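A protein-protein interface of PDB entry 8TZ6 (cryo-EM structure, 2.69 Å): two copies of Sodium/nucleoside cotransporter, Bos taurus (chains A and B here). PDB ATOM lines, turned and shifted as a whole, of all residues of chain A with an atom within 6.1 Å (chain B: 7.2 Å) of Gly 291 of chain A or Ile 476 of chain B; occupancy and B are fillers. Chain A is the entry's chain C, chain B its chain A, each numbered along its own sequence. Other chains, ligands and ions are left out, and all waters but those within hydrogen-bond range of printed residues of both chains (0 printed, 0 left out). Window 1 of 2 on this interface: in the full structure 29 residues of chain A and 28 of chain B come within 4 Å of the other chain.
Printed residues of chain A that touch a printed residue of chain B: Tyr 287, Ser 288, Gly 291, Phe 294, Val 295, Ile 314 and Phe 315.
Hydrophobic or aromatic side chains of chain A within 4 Å of the printed part of chain B: Tyr 287, Phe 294, Val 295, Ile 314 and Phe 315.
Among the printed residues, 11 pairs touch across the chains.
Among the printed residues, no Asp or Glu carboxylate lies within 4 Å of a Lys or Arg side-chain nitrogen of the other chain.
Among the printed residues, merely in contact across the chains: Tyr 287 of chain A with Ala 480 of chain B, Tyr 287 of chain A with Ser 483 of chain B, Ser 288 of chain A with Ala 480 of chain B, Gly 291 of chain A with Ile 476 of chain B, Phe 294 of chain A with Leu 475 of chain B, Phe 294 of chain A with Leu 479 of chain B, Val 295 of chain A with Ala 472 of chain B, Val 295 of chain A with Ile 476 of chain B, Ile 314 of chain A with Val 473 of chain B, Phe 315 of chain A with Ala 480 of chain B and Phe 315 of chain A with Leu 481 of chain B.
No position is printed for both chains.
No residue of chain B comes within 4 Å of Ala 290 of chain A.
Of chain B, only Ile 476 (3.8 Å) comes within 4 Å of Gly 291 of chain A.
Printed residues of chain B within 4 Å of Phe 294 of chain A: Leu 475 (3.7 Å) and Leu 479 (3.97 Å).
Of the printed residues of chain B, Ile 314 of chain A touches Val 473 (3.4 Å).
Asn 470 of chain B touches none of the printed residues of chain A.
Printed residues of chain A within 4 Å of Leu 475 of chain B: Phe 294 (3.7 Å).
Of the printed residues of chain A, Ile 476 of chain B touches Gly 291 (3.8 Å) and Val 295 (3.7 Å).
Printed residues of chain A within 4 Å of Ala 480 of chain B: Tyr 287, Ser 288 and Phe 315.
The nearest residue of chain B that does not touch Gly 291 of chain A is Leu 479 of chain B (4.05 Å).
The nearest printed residue of chain A that does not touch Ile 476 of chain B is Phe 296 of chain A (4.2 Å).
The nearest printed residue of chain A that does not touch Leu 479 of chain B is Gly 291 of chain A (4.05 Å).
O of Leu 479 of chain B is in hydrogen-bond range of OG of Ser 483 of chain B (3.4 Å).
OG of Ser 483 of chain B sits at hydrogen-bond distance from O of Ala 480 of chain B (2.5 Å).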
ATOM      1  N   TYR A 287     -28.227  -8.852   2.533  1.00  0.00           N
ATOM      2  CA  TYR A 287     -27.878  -7.505   2.964  1.00  0.00           C
ATOM      3  C   TYR A 287     -27.164  -6.718   1.875  1.00  0.00           C
ATOM      4  O   TYR A 287     -27.208  -5.484   1.881  1.00  0.00           O
ATOM      5  CB  TYR A 287     -27.010  -7.572   4.219  1.00  0.00           C
ATOM      6  CG  TYR A 287     -27.726  -8.092   5.445  1.00  0.00           C
ATOM      7  CD1 TYR A 287     -29.002  -7.657   5.767  1.00  0.00           C
ATOM      8  CD2 TYR A 287     -27.126  -9.020   6.277  1.00  0.00           C
ATOM      9  CE1 TYR A 287     -29.654  -8.128   6.881  1.00  0.00           C
ATOM     10  CE2 TYR A 287     -27.772  -9.498   7.396  1.00  0.00           C
ATOM     11  CZ  TYR A 287     -29.036  -9.048   7.691  1.00  0.00           C
ATOM     12  OH  TYR A 287     -29.689  -9.518   8.804  1.00  0.00           O
ATOM     13  N   SER A 288     -26.502  -7.404   0.941  1.00  0.00           N
ATOM     14  CA  SER A 288     -25.808  -6.719  -0.142  1.00  0.00           C
ATOM     15  C   SER A 288     -26.765  -5.993  -1.078  1.00  0.00           C
ATOM     16  O   SER A 288     -26.326  -5.136  -1.859  1.00  0.00           O
ATOM     17  CB  SER A 288     -24.972  -7.724  -0.930  1.00  0.00           C
ATOM     18  OG  SER A 288     -25.781  -8.759  -1.450  1.00  0.00           O
ATOM     19  N   ASP A 289     -28.057  -6.324  -1.017  1.00  0.00           N
ATOM     20  CA  ASP A 289     -29.027  -5.691  -1.899  1.00  0.00           C
ATOM     21  C   ASP A 289     -29.121  -4.195  -1.648  1.00  0.00           C
ATOM     22  O   ASP A 289     -29.412  -3.436  -2.572  1.00  0.00           O
ATOM     23  CB  ASP A 289     -30.396  -6.342  -1.728  1.00  0.00           C
ATOM     24  CG  ASP A 289     -30.430  -7.767  -2.236  1.00  0.00           C
ATOM     25  OD1 ASP A 289     -29.391  -8.247  -2.733  1.00  0.00           O
ATOM     26  OD2 ASP A 289     -31.496  -8.408  -2.139  1.00  0.00           O
ATOM     27  N   ALA A 290     -28.860  -3.748  -0.420  1.00  0.00           N
ATOM     28  CA  ALA A 290     -28.899  -2.318  -0.133  1.00  0.00           C
ATOM     29  C   ALA A 290     -27.841  -1.569  -0.935  1.00  0.00           C
ATOM     30  O   ALA A 290     -28.138  -0.579  -1.623  1.00  0.00           O
ATOM     31  CB  ALA A 290     -28.703  -2.095   1.363  1.00  0.00           C
ATOM     32  N   GLY A 291     -26.595  -2.037  -0.867  1.00  0.00           N
ATOM     33  CA  GLY A 291     -25.535  -1.405  -1.629  1.00  0.00           C
ATOM     34  C   GLY A 291     -25.747  -1.530  -3.123  1.00  0.00           C
ATOM     35  O   GLY A 291     -25.515  -0.577  -3.875  1.00  0.00           O
ATOM     36  N   ALA A 292     -26.197  -2.701  -3.576  1.00  0.00           N
ATOM     37  CA  ALA A 292     -26.452  -2.877  -5.000  1.00  0.00           C
ATOM     38  C   ALA A 292     -27.539  -1.928  -5.484  1.00  0.00           C
ATOM     39  O   ALA A 292     -27.437  -1.360  -6.577  1.00  0.00           O
ATOM     40  CB  ALA A 292     -26.833  -4.325  -5.287  1.00  0.00           C
ATOM     41  N   SER A 293     -28.588  -1.741  -4.682  1.00  0.00           N
ATOM     42  CA  SER A 293     -29.673  -0.846  -5.058  1.00  0.00           C
ATOM     43  C   SER A 293     -29.203   0.597  -5.120  1.00  0.00           C
ATOM     44  O   SER A 293     -29.562   1.328  -6.049  1.00  0.00           O
ATOM     45  CB  SER A 293     -30.824  -0.988  -4.068  1.00  0.00           C
ATOM     46  OG  SER A 293     -31.944  -0.226  -4.473  1.00  0.00           O
ATOM     47  N   PHE A 294     -28.410   1.036  -4.142  1.00  0.00           N
ATOM     48  CA  PHE A 294     -27.937   2.415  -4.186  1.00  0.00           C
ATOM     49  C   PHE A 294     -27.019   2.644  -5.377  1.00  0.00           C
ATOM     50  O   PHE A 294     -27.218   3.585  -6.154  1.00  0.00           O
ATOM     51  CB  PHE A 294     -27.219   2.790  -2.894  1.00  0.00           C
ATOM     52  CG  PHE A 294     -26.571   4.144  -2.947  1.00  0.00           C
ATOM     53  CD1 PHE A 294     -27.335   5.285  -3.122  1.00  0.00           C
ATOM     54  CD2 PHE A 294     -25.200   4.277  -2.840  1.00  0.00           C
ATOM     55  CE1 PHE A 294     -26.744   6.528  -3.183  1.00  0.00           C
ATOM     56  CE2 PHE A 294     -24.605   5.520  -2.898  1.00  0.00           C
ATOM     57  CZ  PHE A 294     -25.378   6.645  -3.070  1.00  0.00           C
ATOM     58  N   VAL A 295     -26.006   1.792  -5.543  1.00  0.00           N
ATOM     59  CA  VAL A 295     -25.019   2.023  -6.592  1.00  0.00           C
ATOM     60  C   VAL A 295     -25.645   1.845  -7.969  1.00  0.00           C
ATOM     61  O   VAL A 295     -25.425   2.657  -8.876  1.00  0.00           O
ATOM     62  CB  VAL A 295     -23.806   1.098  -6.396  1.00  0.00           C
ATOM     63  CG1 VAL A 295     -22.799   1.311  -7.495  1.00  0.00           C
ATOM     64  CG2 VAL A 295     -23.164   1.358  -5.060  1.00  0.00           C
ATOM     65  N   PHE A 296     -26.436   0.790  -8.149  1.00  0.00           N
ATOM     66  CA  PHE A 296     -26.982   0.441  -9.453  1.00  0.00           C
ATOM     67  C   PHE A 296     -28.473   0.722  -9.579  1.00  0.00           C
ATOM     68  O   PHE A 296     -29.069   0.374 -10.603  1.00  0.00           O
ATOM     69  CB  PHE A 296     -26.702  -1.031  -9.751  1.00  0.00           C
ATOM     70  CG  PHE A 296     -25.249  -1.388  -9.700  1.00  0.00           C
ATOM     71  CD1 PHE A 296     -24.348  -0.815 -10.576  1.00  0.00           C
ATOM     72  CD2 PHE A 296     -24.783  -2.302  -8.778  1.00  0.00           C
ATOM     73  CE1 PHE A 296     -23.017  -1.145 -10.528  1.00  0.00           C
ATOM     74  CE2 PHE A 296     -23.454  -2.634  -8.731  1.00  0.00           C
ATOM     75  CZ  PHE A 296     -22.571  -2.055  -9.606  1.00  0.00           C
ATOM     76  N   PRO A 311     -22.021  -8.386  -6.087  1.00  0.00           N
ATOM     77  CA  PRO A 311     -22.007  -7.712  -4.782  1.00  0.00           C
ATOM     78  C   PRO A 311     -22.038  -8.670  -3.608  1.00  0.00           C
ATOM     79  O   PRO A 311     -21.494  -8.354  -2.544  1.00  0.00           O
ATOM     80  CB  PRO A 311     -23.263  -6.840  -4.843  1.00  0.00           C
ATOM     81  CG  PRO A 311     -23.412  -6.525  -6.274  1.00  0.00           C
ATOM     82  CD  PRO A 311     -22.946  -7.731  -7.027  1.00  0.00           C
ATOM     83  N   ILE A 314     -18.510  -9.502  -3.106  1.00  0.00           N
ATOM     84  CA  ILE A 314     -17.827  -8.378  -2.467  1.00  0.00           C
ATOM     85  C   ILE A 314     -18.085  -8.379  -0.965  1.00  0.00           C
ATOM     86  O   ILE A 314     -17.159  -8.273  -0.149  1.00  0.00           O
ATOM     87  CB  ILE A 314     -18.277  -7.057  -3.114  1.00  0.00           C
ATOM     88  CG1 ILE A 314     -17.792  -6.985  -4.559  1.00  0.00           C
ATOM     89  CG2 ILE A 314     -17.775  -5.878  -2.316  1.00  0.00           C
ATOM     90  CD1 ILE A 314     -18.425  -5.888  -5.362  1.00  0.00           C
ATOM     91  N   PHE A 315     -19.358  -8.490  -0.581  1.00  0.00           N
ATOM     92  CA  PHE A 315     -19.724  -8.441   0.828  1.00  0.00           C
ATOM     93  C   PHE A 315     -19.120  -9.607   1.599  1.00  0.00           C
ATOM     94  O   PHE A 315     -18.629  -9.433   2.722  1.00  0.00           O
ATOM     95  CB  PHE A 315     -21.246  -8.429   0.952  1.00  0.00           C
ATOM     96  CG  PHE A 315     -21.747  -8.416   2.361  1.00  0.00           C
ATOM     97  CD1 PHE A 315     -21.230  -7.534   3.289  1.00  0.00           C
ATOM     98  CD2 PHE A 315     -22.756  -9.275   2.753  1.00  0.00           C
ATOM     99  CE1 PHE A 315     -21.696  -7.522   4.580  1.00  0.00           C
ATOM    100  CE2 PHE A 315     -23.225  -9.263   4.041  1.00  0.00           C
ATOM    101  CZ  PHE A 315     -22.697  -8.388   4.956  1.00  0.00           C
ATOM    102  N   ASN B 470     -13.186   1.755  -6.375  1.00  0.00           N
ATOM    103  CA  ASN B 470     -13.139   1.681  -4.922  1.00  0.00           C
ATOM    104  C   ASN B 470     -14.332   2.384  -4.293  1.00  0.00           C
ATOM    105  O   ASN B 470     -14.900   1.891  -3.313  1.00  0.00           O
ATOM    106  CB  ASN B 470     -11.829   2.275  -4.412  1.00  0.00           C
ATOM    107  CG  ASN B 470     -10.675   1.300  -4.500  1.00  0.00           C
ATOM    108  OD1 ASN B 470     -10.477   0.475  -3.611  1.00  0.00           O
ATOM    109  ND2 ASN B 470      -9.904   1.392  -5.571  1.00  0.00           N
ATOM    110  N   ILE B 471     -14.733   3.536  -4.837  1.00  0.00           N
ATOM    111  CA  ILE B 471     -15.902   4.231  -4.302  1.00  0.00           C
ATOM    112  C   ILE B 471     -17.112   3.306  -4.317  1.00  0.00           C
ATOM    113  O   ILE B 471     -17.799   3.129  -3.303  1.00  0.00           O
ATOM    114  CB  ILE B 471     -16.170   5.521  -5.097  1.00  0.00           C
ATOM    115  CG1 ILE B 471     -15.133   6.593  -4.756  1.00  0.00           C
ATOM    116  CG2 ILE B 471     -17.574   6.034  -4.827  1.00  0.00           C
ATOM    117  CD1 ILE B 471     -15.190   7.808  -5.651  1.00  0.00           C
ATOM    118  N   ALA B 472     -17.370   2.679  -5.466  1.00  0.00           N
ATOM    119  CA  ALA B 472     -18.553   1.838  -5.604  1.00  0.00           C
ATOM    120  C   ALA B 472     -18.497   0.637  -4.669  1.00  0.00           C
ATOM    121  O   ALA B 472     -19.474   0.329  -3.972  1.00  0.00           O
ATOM    122  CB  ALA B 472     -18.692   1.383  -7.053  1.00  0.00           C
ATOM    123  N   VAL B 473     -17.359  -0.060  -4.643  1.00  0.00           N
ATOM    124  CA  VAL B 473     -17.263  -1.267  -3.828  1.00  0.00           C
ATOM    125  C   VAL B 473     -17.380  -0.930  -2.345  1.00  0.00           C
ATOM    126  O   VAL B 473     -18.067  -1.631  -1.588  1.00  0.00           O
ATOM    127  CB  VAL B 473     -15.957  -2.014  -4.148  1.00  0.00           C
ATOM    128  CG1 VAL B 473     -15.849  -3.273  -3.343  1.00  0.00           C
ATOM    129  CG2 VAL B 473     -15.916  -2.376  -5.602  1.00  0.00           C
ATOM    130  N   ASN B 474     -16.702   0.128  -1.899  1.00  0.00           N
ATOM    131  CA  ASN B 474     -16.784   0.515  -0.498  1.00  0.00           C
ATOM    132  C   ASN B 474     -18.199   0.926  -0.123  1.00  0.00           C
ATOM    133  O   ASN B 474     -18.666   0.617   0.976  1.00  0.00           O
ATOM    134  CB  ASN B 474     -15.796   1.643  -0.206  1.00  0.00           C
ATOM    135  CG  ASN B 474     -14.403   1.133   0.077  1.00  0.00           C
ATOM    136  OD1 ASN B 474     -14.008   0.984   1.230  1.00  0.00           O
ATOM    137  ND2 ASN B 474     -13.650   0.853  -0.977  1.00  0.00           N
ATOM    138  N   LEU B 475     -18.899   1.629  -1.016  1.00  0.00           N
ATOM    139  CA  LEU B 475     -20.288   1.968  -0.732  1.00  0.00           C
ATOM    140  C   LEU B 475     -21.137   0.716  -0.571  1.00  0.00           C
ATOM    141  O   LEU B 475     -21.935   0.610   0.370  1.00  0.00           O
ATOM    142  CB  LEU B 475     -20.848   2.853  -1.841  1.00  0.00           C
ATOM    143  CG  LEU B 475     -20.536   4.340  -1.727  1.00  0.00           C
ATOM    144  CD1 LEU B 475     -20.936   5.045  -2.990  1.00  0.00           C
ATOM    145  CD2 LEU B 475     -21.258   4.941  -0.547  1.00  0.00           C
ATOM    146  N   ILE B 476     -20.970  -0.251  -1.474  1.00  0.00           N
ATOM    147  CA  ILE B 476     -21.738  -1.489  -1.375  1.00  0.00           C
ATOM    148  C   ILE B 476     -21.496  -2.149  -0.024  1.00  0.00           C
ATOM    149  O   ILE B 476     -22.439  -2.486   0.709  1.00  0.00           O
ATOM    150  CB  ILE B 476     -21.372  -2.438  -2.531  1.00  0.00           C
ATOM    151  CG1 ILE B 476     -21.908  -1.899  -3.854  1.00  0.00           C
ATOM    152  CG2 ILE B 476     -21.902  -3.831  -2.260  1.00  0.00           C
ATOM    153  CD1 ILE B 476     -21.460  -2.671  -5.058  1.00  0.00           C
ATOM    154  N   ALA B 477     -20.223  -2.327   0.331  1.00  0.00           N
ATOM    155  CA  ALA B 477     -19.892  -3.027   1.566  1.00  0.00           C
ATOM    156  C   ALA B 477     -20.396  -2.271   2.788  1.00  0.00           C
ATOM    157  O   ALA B 477     -20.952  -2.874   3.713  1.00  0.00           O
ATOM    158  CB  ALA B 477     -18.385  -3.241   1.651  1.00  0.00           C
ATOM    159  N   PHE B 478     -20.208  -0.950   2.815  1.00  0.00           N
ATOM    160  CA  PHE B 478     -20.623  -0.167   3.972  1.00  0.00           C
ATOM    161  C   PHE B 478     -22.130  -0.210   4.164  1.00  0.00           C
ATOM    162  O   PHE B 478     -22.610  -0.353   5.293  1.00  0.00           O
ATOM    163  CB  PHE B 478     -20.145   1.279   3.827  1.00  0.00           C
ATOM    164  CG  PHE B 478     -18.676   1.479   4.095  1.00  0.00           C
ATOM    165  CD1 PHE B 478     -17.970   0.623   4.926  1.00  0.00           C
ATOM    166  CD2 PHE B 478     -18.001   2.539   3.517  1.00  0.00           C
ATOM    167  CE1 PHE B 478     -16.631   0.818   5.166  1.00  0.00           C
ATOM    168  CE2 PHE B 478     -16.658   2.735   3.757  1.00  0.00           C
ATOM    169  CZ  PHE B 478     -15.975   1.875   4.582  1.00  0.00           C
ATOM    170  N   LEU B 479     -22.900  -0.083   3.083  1.00  0.00           N
ATOM    171  CA  LEU B 479     -24.349  -0.100   3.245  1.00  0.00           C
ATOM    172  C   LEU B 479     -24.848  -1.485   3.640  1.00  0.00           C
ATOM    173  O   LEU B 479     -25.779  -1.609   4.448  1.00  0.00           O
ATOM    174  CB  LEU B 479     -25.032   0.388   1.973  1.00  0.00           C
ATOM    175  CG  LEU B 479     -25.145   1.909   1.858  1.00  0.00           C
ATOM    176  CD1 LEU B 479     -23.853   2.508   1.385  1.00  0.00           C
ATOM    177  CD2 LEU B 479     -26.260   2.307   0.928  1.00  0.00           C
ATOM    178  N   ALA B 480     -24.234  -2.543   3.101  1.00  0.00           N
ATOM    179  CA  ALA B 480     -24.598  -3.887   3.541  1.00  0.00           C
ATOM    180  C   ALA B 480     -24.310  -4.082   5.027  1.00  0.00           C
ATOM    181  O   ALA B 480     -25.137  -4.637   5.765  1.00  0.00           O
ATOM    182  CB  ALA B 480     -23.849  -4.921   2.708  1.00  0.00           C
ATOM    183  N   LEU B 481     -23.140  -3.629   5.485  1.00  0.00           N
ATOM    184  CA  LEU B 481     -22.809  -3.727   6.903  1.00  0.00           C
ATOM    185  C   LEU B 481     -23.774  -2.918   7.755  1.00  0.00           C
ATOM    186  O   LEU B 481     -24.147  -3.344   8.851  1.00  0.00           O
ATOM    187  CB  LEU B 481     -21.379  -3.254   7.138  1.00  0.00           C
ATOM    188  CG  LEU B 481     -20.272  -4.189   6.668  1.00  0.00           C
ATOM    189  CD1 LEU B 481     -18.951  -3.464   6.679  1.00  0.00           C
ATOM    190  CD2 LEU B 481     -20.209  -5.413   7.550  1.00  0.00           C
ATOM    191  N   LEU B 482     -24.166  -1.736   7.283  1.00  0.00           N
ATOM    192  CA  LEU B 482     -25.127  -0.924   8.019  1.00  0.00           C
ATOM    193  C   LEU B 482     -26.452  -1.657   8.175  1.00  0.00           C
ATOM    194  O   LEU B 482     -27.038  -1.684   9.264  1.00  0.00           O
ATOM    195  CB  LEU B 482     -25.323   0.410   7.302  1.00  0.00           C
ATOM    196  CG  LEU B 482     -26.315   1.402   7.899  1.00  0.00           C
ATOM    197  CD1 LEU B 482     -25.927   1.775   9.307  1.00  0.00           C
ATOM    198  CD2 LEU B 482     -26.382   2.631   7.030  1.00  0.00           C
ATOM    199  N   SER B 483     -26.939  -2.265   7.091  1.00  0.00           N
ATOM    200  CA  SER B 483     -28.189  -3.015   7.173  1.00  0.00           C
ATOM    201  C   SER B 483     -28.072  -4.172   8.156  1.00  0.00           C
ATOM    202  O   SER B 483     -28.969  -4.390   8.983  1.00  0.00           O
ATOM    203  CB  SER B 483     -28.580  -3.528   5.790  1.00  0.00           C
ATOM    204  OG  SER B 483     -27.593  -4.402   5.284  1.00  0.00           O
